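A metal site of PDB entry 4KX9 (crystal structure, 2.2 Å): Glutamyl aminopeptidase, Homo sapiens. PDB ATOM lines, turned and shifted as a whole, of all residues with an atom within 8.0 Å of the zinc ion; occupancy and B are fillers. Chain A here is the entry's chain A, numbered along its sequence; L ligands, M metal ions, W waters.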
ATOM      1  N   GLU A 148     -20.220  22.019 -22.823  1.00  0.00           N
ATOM      2  CA  GLU A 148     -20.352  20.971 -21.792  1.00  0.00           C
ATOM      3  C   GLU A 148     -20.421  19.556 -22.369  1.00  0.00           C
ATOM      4  O   GLU A 148     -21.258  19.276 -23.218  1.00  0.00           O
ATOM      5  CB  GLU A 148     -21.546  21.230 -20.866  1.00  0.00           C
ATOM      6  CG  GLU A 148     -21.532  20.357 -19.612  1.00  0.00           C
ATOM      7  CD  GLU A 148     -22.573  20.744 -18.580  1.00  0.00           C
ATOM      8  OE1 GLU A 148     -23.650  21.288 -18.933  1.00  0.00           O
ATOM      9  OE2 GLU A 148     -22.318  20.458 -17.386  1.00  0.00           O
ATOM     10  N   ALA A 283     -30.655  22.343 -23.945  1.00  0.00           N
ATOM     11  CA  ALA A 283     -30.318  23.696 -23.555  1.00  0.00           C
ATOM     12  C   ALA A 283     -29.018  23.654 -22.762  1.00  0.00           C
ATOM     13  O   ALA A 283     -28.627  22.589 -22.266  1.00  0.00           O
ATOM     14  CB  ALA A 283     -31.428  24.307 -22.710  1.00  0.00           C
ATOM     15  N   MET A 284     -28.353  24.803 -22.633  1.00  0.00           N
ATOM     16  CA  MET A 284     -27.089  24.885 -21.909  1.00  0.00           C
ATOM     17  C   MET A 284     -27.054  26.123 -21.013  1.00  0.00           C
ATOM     18  O   MET A 284     -27.332  27.230 -21.459  1.00  0.00           O
ATOM     19  CB  MET A 284     -25.916  24.877 -22.891  1.00  0.00           C
ATOM     20  CG  MET A 284     -24.574  24.894 -22.202  1.00  0.00           C
ATOM     21  SD  MET A 284     -24.467  23.624 -20.918  1.00  0.00           S
ATOM     22  CE  MET A 284     -23.165  24.349 -19.924  1.00  0.00           C
ATOM     23  N   GLU A 285     -26.658  25.926 -19.749  1.00  0.00           N
ATOM     24  CA  GLU A 285     -26.837  26.931 -18.713  1.00  0.00           C
ATOM     25  C   GLU A 285     -25.760  28.020 -18.651  1.00  0.00           C
ATOM     26  O   GLU A 285     -25.554  28.617 -17.588  1.00  0.00           O
ATOM     27  CB  GLU A 285     -26.926  26.246 -17.342  1.00  0.00           C
ATOM     28  CG  GLU A 285     -25.643  25.557 -16.892  1.00  0.00           C
ATOM     29  CD  GLU A 285     -25.573  24.083 -17.229  1.00  0.00           C
ATOM     30  OE1 GLU A 285     -26.120  23.640 -18.267  1.00  0.00           O
ATOM     31  OE2 GLU A 285     -24.937  23.348 -16.451  1.00  0.00           O
ATOM     32  N   VAL A 315     -37.791  23.465 -18.840  1.00  0.00           N
ATOM     33  CA  VAL A 315     -36.399  23.633 -19.284  1.00  0.00           C
ATOM     34  C   VAL A 315     -35.875  25.026 -18.876  1.00  0.00           C
ATOM     35  O   VAL A 315     -34.763  25.151 -18.378  1.00  0.00           O
ATOM     36  CB  VAL A 315     -36.229  23.394 -20.790  1.00  0.00           C
ATOM     37  CG1 VAL A 315     -34.776  23.569 -21.193  1.00  0.00           C
ATOM     38  CG2 VAL A 315     -36.667  21.997 -21.169  1.00  0.00           C
ATOM     39  N   HIS A 318     -35.269  24.714 -15.271  1.00  0.00           N
ATOM     40  CA  HIS A 318     -34.072  23.875 -15.137  1.00  0.00           C
ATOM     41  C   HIS A 318     -32.828  24.734 -15.300  1.00  0.00           C
ATOM     42  O   HIS A 318     -31.941  24.729 -14.437  1.00  0.00           O
ATOM     43  CB  HIS A 318     -34.087  22.749 -16.191  1.00  0.00           C
ATOM     44  CG  HIS A 318     -32.946  21.774 -16.075  1.00  0.00           C
ATOM     45  ND1 HIS A 318     -33.083  20.554 -15.452  1.00  0.00           N
ATOM     46  CD2 HIS A 318     -31.671  21.835 -16.510  1.00  0.00           C
ATOM     47  CE1 HIS A 318     -31.930  19.907 -15.505  1.00  0.00           C
ATOM     48  NE2 HIS A 318     -31.059  20.666 -16.139  1.00  0.00           N
ATOM     49  N   GLU A 319     -32.789  25.484 -16.395  1.00  0.00           N
ATOM     50  CA  GLU A 319     -31.657  26.307 -16.750  1.00  0.00           C
ATOM     51  C   GLU A 319     -31.410  27.383 -15.706  1.00  0.00           C
ATOM     52  O   GLU A 319     -30.268  27.711 -15.387  1.00  0.00           O
ATOM     53  CB  GLU A 319     -31.848  26.942 -18.134  1.00  0.00           C
ATOM     54  CG  GLU A 319     -31.876  25.949 -19.292  1.00  0.00           C
ATOM     55  CD  GLU A 319     -30.836  24.852 -19.177  1.00  0.00           C
ATOM     56  OE1 GLU A 319     -29.657  25.171 -18.965  1.00  0.00           O
ATOM     57  OE2 GLU A 319     -31.192  23.677 -19.319  1.00  0.00           O
ATOM     58  N   VAL A 321     -32.161  27.181 -12.476  1.00  0.00           N
ATOM     59  CA  VAL A 321     -31.619  26.553 -11.268  1.00  0.00           C
ATOM     60  C   VAL A 321     -30.097  26.520 -11.344  1.00  0.00           C
ATOM     61  O   VAL A 321     -29.419  26.767 -10.355  1.00  0.00           O
ATOM     62  CB  VAL A 321     -32.127  25.105 -11.052  1.00  0.00           C
ATOM     63  CG1 VAL A 321     -31.490  24.499  -9.820  1.00  0.00           C
ATOM     64  CG2 VAL A 321     -33.633  25.082 -10.911  1.00  0.00           C
ATOM     65  N   HIS A 322     -29.580  26.221 -12.519  1.00  0.00           N
ATOM     66  CA  HIS A 322     -28.139  26.113 -12.717  1.00  0.00           C
ATOM     67  C   HIS A 322     -27.373  27.392 -12.404  1.00  0.00           C
ATOM     68  O   HIS A 322     -26.193  27.343 -12.060  1.00  0.00           O
ATOM     69  CB  HIS A 322     -27.822  25.659 -14.129  1.00  0.00           C
ATOM     70  CG  HIS A 322     -27.906  24.165 -14.338  1.00  0.00           C
ATOM     71  ND1 HIS A 322     -27.164  23.267 -13.610  1.00  0.00           N
ATOM     72  CD2 HIS A 322     -28.626  23.432 -15.216  1.00  0.00           C
ATOM     73  CE1 HIS A 322     -27.430  22.044 -14.025  1.00  0.00           C
ATOM     74  NE2 HIS A 322     -28.304  22.115 -15.008  1.00  0.00           N
ATOM     75  N   PHE A 325     -27.076  26.286  -8.705  1.00  0.00           N
ATOM     76  CA  PHE A 325     -26.454  24.968  -8.614  1.00  0.00           C
ATOM     77  C   PHE A 325     -25.824  24.548  -9.936  1.00  0.00           C
ATOM     78  O   PHE A 325     -26.503  24.128 -10.865  1.00  0.00           O
ATOM     79  CB  PHE A 325     -27.448  23.917  -8.123  1.00  0.00           C
ATOM     80  CG  PHE A 325     -27.797  24.084  -6.674  1.00  0.00           C
ATOM     81  CD1 PHE A 325     -27.021  23.474  -5.697  1.00  0.00           C
ATOM     82  CD2 PHE A 325     -28.872  24.857  -6.290  1.00  0.00           C
ATOM     83  CE1 PHE A 325     -27.332  23.632  -4.355  1.00  0.00           C
ATOM     84  CE2 PHE A 325     -29.197  25.018  -4.956  1.00  0.00           C
ATOM     85  CZ  PHE A 325     -28.417  24.400  -3.979  1.00  0.00           C
ATOM     86  N   LEU A 337     -21.330  15.009 -10.872  1.00  0.00           N
ATOM     87  CA  LEU A 337     -22.228  15.707 -11.820  1.00  0.00           C
ATOM     88  C   LEU A 337     -23.660  15.907 -11.318  1.00  0.00           C
ATOM     89  O   LEU A 337     -24.269  16.940 -11.584  1.00  0.00           O
ATOM     90  CB  LEU A 337     -22.256  15.002 -13.173  1.00  0.00           C
ATOM     91  CG  LEU A 337     -23.168  15.555 -14.285  1.00  0.00           C
ATOM     92  CD1 LEU A 337     -22.798  16.989 -14.662  1.00  0.00           C
ATOM     93  CD2 LEU A 337     -23.100  14.646 -15.498  1.00  0.00           C
ATOM     94  N   ASN A 340     -24.990  19.076  -9.938  1.00  0.00           N
ATOM     95  CA  ASN A 340     -25.504  20.021 -10.921  1.00  0.00           C
ATOM     96  C   ASN A 340     -26.860  19.568 -11.417  1.00  0.00           C
ATOM     97  O   ASN A 340     -27.871  20.241 -11.215  1.00  0.00           O
ATOM     98  CB  ASN A 340     -24.547  20.127 -12.116  1.00  0.00           C
ATOM     99  CG  ASN A 340     -23.365  21.042 -11.858  1.00  0.00           C
ATOM    100  OD1 ASN A 340     -22.805  21.616 -12.790  1.00  0.00           O
ATOM    101  ND2 ASN A 340     -22.965  21.186 -10.602  1.00  0.00           N
ATOM    102  N   GLU A 341     -26.870  18.396 -12.050  1.00  0.00           N
ATOM    103  CA  GLU A 341     -28.017  17.947 -12.823  1.00  0.00           C
ATOM    104  C   GLU A 341     -29.209  17.468 -12.008  1.00  0.00           C
ATOM    105  O   GLU A 341     -30.351  17.730 -12.362  1.00  0.00           O
ATOM    106  CB  GLU A 341     -27.593  16.909 -13.872  1.00  0.00           C
ATOM    107  CG  GLU A 341     -26.479  17.393 -14.787  1.00  0.00           C
ATOM    108  CD  GLU A 341     -26.850  18.618 -15.608  1.00  0.00           C
ATOM    109  OE1 GLU A 341     -28.038  18.935 -15.737  1.00  0.00           O
ATOM    110  OE2 GLU A 341     -25.937  19.281 -16.136  1.00  0.00           O
ATOM    111  N   GLY A 342     -28.921  16.754 -10.925  1.00  0.00           N
ATOM    112  CA  GLY A 342     -29.961  16.269 -10.032  1.00  0.00           C
ATOM    113  C   GLY A 342     -30.679  17.423  -9.358  1.00  0.00           C
ATOM    114  O   GLY A 342     -31.900  17.428  -9.233  1.00  0.00           O
ATOM    115  N   PHE A 343     -29.900  18.415  -8.945  1.00  0.00           N
ATOM    116  CA  PHE A 343     -30.434  19.617  -8.304  1.00  0.00           C
ATOM    117  C   PHE A 343     -31.309  20.447  -9.238  1.00  0.00           C
ATOM    118  O   PHE A 343     -32.392  20.887  -8.847  1.00  0.00           O
ATOM    119  CB  PHE A 343     -29.311  20.464  -7.713  1.00  0.00           C
ATOM    120  CG  PHE A 343     -28.751  19.903  -6.434  1.00  0.00           C
ATOM    121  CD1 PHE A 343     -28.048  18.704  -6.450  1.00  0.00           C
ATOM    122  CD2 PHE A 343     -28.943  20.557  -5.236  1.00  0.00           C
ATOM    123  CE1 PHE A 343     -27.550  18.165  -5.266  1.00  0.00           C
ATOM    124  CE2 PHE A 343     -28.431  20.035  -4.056  1.00  0.00           C
ATOM    125  CZ  PHE A 343     -27.739  18.832  -4.080  1.00  0.00           C
ATOM    126  N   ALA A 344     -30.841  20.638 -10.471  1.00  0.00           N
ATOM    127  CA  ALA A 344     -31.625  21.319 -11.494  1.00  0.00           C
ATOM    128  C   ALA A 344     -32.900  20.536 -11.814  1.00  0.00           C
ATOM    129  O   ALA A 344     -33.980  21.121 -11.928  1.00  0.00           O
ATOM    130  CB  ALA A 344     -30.804  21.559 -12.745  1.00  0.00           C
ATOM    131  N   SER A 345     -32.776  19.215 -11.942  1.00  0.00           N
ATOM    132  CA  SER A 345     -33.929  18.335 -12.199  1.00  0.00           C
ATOM    133  C   SER A 345     -34.943  18.312 -11.044  1.00  0.00           C
ATOM    134  O   SER A 345     -36.129  18.055 -11.263  1.00  0.00           O
ATOM    135  CB  SER A 345     -33.489  16.906 -12.536  1.00  0.00           C
ATOM    136  OG  SER A 345     -32.756  16.856 -13.751  1.00  0.00           O
ATOM    137  N   GLU A 348     -36.385  22.383 -10.734  1.00  0.00           N
ATOM    138  CA  GLU A 348     -37.168  22.761 -11.918  1.00  0.00           C
ATOM    139  C   GLU A 348     -38.659  22.675 -11.620  1.00  0.00           C
ATOM    140  O   GLU A 348     -39.422  23.532 -12.046  1.00  0.00           O
ATOM    141  CB  GLU A 348     -36.781  21.929 -13.147  1.00  0.00           C
ATOM    142  CG  GLU A 348     -37.274  20.501 -13.148  1.00  0.00           C
ATOM    143  CD  GLU A 348     -36.848  19.709 -14.368  1.00  0.00           C
ATOM    144  OE1 GLU A 348     -37.544  18.735 -14.714  1.00  0.00           O
ATOM    145  OE2 GLU A 348     -35.812  20.029 -14.978  1.00  0.00           O
ATOM    146  N   PHE A 399     -24.207  12.035 -18.328  1.00  0.00           N
ATOM    147  CA  PHE A 399     -25.339  12.946 -18.480  1.00  0.00           C
ATOM    148  C   PHE A 399     -26.558  12.099 -18.832  1.00  0.00           C
ATOM    149  O   PHE A 399     -26.967  12.042 -19.994  1.00  0.00           O
ATOM    150  CB  PHE A 399     -25.038  13.991 -19.557  1.00  0.00           C
ATOM    151  CG  PHE A 399     -24.050  15.045 -19.131  1.00  0.00           C
ATOM    152  CD1 PHE A 399     -22.677  14.822 -19.255  1.00  0.00           C
ATOM    153  CD2 PHE A 399     -24.492  16.261 -18.608  1.00  0.00           C
ATOM    154  CE1 PHE A 399     -21.761  15.799 -18.861  1.00  0.00           C
ATOM    155  CE2 PHE A 399     -23.578  17.236 -18.224  1.00  0.00           C
ATOM    156  CZ  PHE A 399     -22.219  16.997 -18.343  1.00  0.00           C
ATOM    157  N   TYR A 404     -29.686  12.799 -13.619  1.00  0.00           N
ATOM    158  CA  TYR A 404     -30.855  13.679 -13.579  1.00  0.00           C
ATOM    159  C   TYR A 404     -32.006  13.142 -12.744  1.00  0.00           C
ATOM    160  O   TYR A 404     -32.423  13.775 -11.773  1.00  0.00           O
ATOM    161  CB  TYR A 404     -31.392  13.928 -14.990  1.00  0.00           C
ATOM    162  CG  TYR A 404     -30.537  14.813 -15.869  1.00  0.00           C
ATOM    163  CD1 TYR A 404     -29.337  14.354 -16.377  1.00  0.00           C
ATOM    164  CD2 TYR A 404     -30.956  16.092 -16.200  1.00  0.00           C
ATOM    165  CE1 TYR A 404     -28.552  15.155 -17.186  1.00  0.00           C
ATOM    166  CE2 TYR A 404     -30.178  16.912 -16.999  1.00  0.00           C
ATOM    167  CZ  TYR A 404     -28.986  16.429 -17.494  1.00  0.00           C
ATOM    168  OH  TYR A 404     -28.210  17.205 -18.288  1.00  0.00           O
HETATM  169  N1  LIG L   1     -26.536  20.296 -19.270  1.00  0.00           N
HETATM  170  C1  LIG L   1     -27.503  20.551 -20.371  1.00  0.00           C
HETATM  171  C2  LIG L   1     -28.946  20.172 -19.978  1.00  0.00           C
HETATM  172  O1  LIG L   1     -29.860  21.002 -19.940  1.00  0.00           O
HETATM  173  C3  LIG L   1     -27.088  19.828 -21.658  1.00  0.00           C
HETATM  174  C4  LIG L   1     -25.602  19.834 -21.996  1.00  0.00           C
HETATM  175  C5  LIG L   1     -25.309  18.717 -22.987  1.00  0.00           C
HETATM  176  N2  LIG L   1     -24.077  18.865 -23.771  1.00  0.00           N
HETATM  177  C6  LIG L   1     -23.801  18.238 -24.934  1.00  0.00           C
HETATM  178  N3  LIG L   1     -24.660  17.391 -25.483  1.00  0.00           N
HETATM  179  N4  LIG L   1     -22.645  18.457 -25.562  1.00  0.00           N
HETATM  180  O2  LIG L   1     -29.216  18.998 -19.695  1.00  0.00           O
HETATM  181 ZN    ZN M   1     -28.777  20.599 -16.540  1.00  0.00          ZN
HETATM  182  O   HOH W   1     -28.253  22.497 -18.508  1.00  0.00           O
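OE2 of Glu 341 lies within salt-bridge range of N1 of the ligand (3.3 Å).
OH of Tyr 404 is in hydrogen-bond range of O2 of the ligand, at 2.5 Å.
The side-chain carboxylate (OE1) of Glu 285 is in salt-bridge range of a nitrogen (N1) of the ligand (3.5 Å).
OE2 of Glu 319 sits close to O1 of the ligand.
O of Glu 148 sits at hydrogen-bond distance from N4 of the ligand (2.8 Å).
The side-chain carboxylate (OE1) of Glu 148 is in salt-bridge range of a nitrogen (N1) of the ligand, 3.1 Å away.
An oxygen (O1) of the ligand lies close to the backbone carbonyl oxygen of Ala 283 (3.1 Å).
The side-chain carboxylate (OE1) of Glu 341 sits close to the side-chain hydroxyl (OH) of Tyr 404.
The backbone carbonyl oxygen of Glu 341 lies within hydrogen-bond range of the side-chain hydroxyl of Ser 345, at 2.9 Å.
ND1 of His 322 is in hydrogen-bond range of O of Phe 325.
A ring nitrogen (ND1) of His 318 lies within hydrogen-bond range of the side-chain carboxylate of Glu 348, at 2.8 Å.
Tyr 404 touches the zinc ion.
Of the 20 residues printed, 4 come within 4 Å of the zinc ion.
The nearest printed residue that does not touch the zinc ion is Glu 285 (4.4 Å).
The zinc ion is bound by the side-chain carboxylate (OE1) of Glu 341, a ring nitrogen (NE2) of His 322 and a ring nitrogen (NE2) of His 318.
Slightly farther from the zinc ion lies water W1 (2.8 Å).
Water W1 lies within hydrogen-bond range of the side-chain carboxylate of Glu 285 (2.4 Å), an oxygen (O1) of the ligand (2.6 Å) and the side-chain carboxylate of Glu 319 (3.1 Å).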
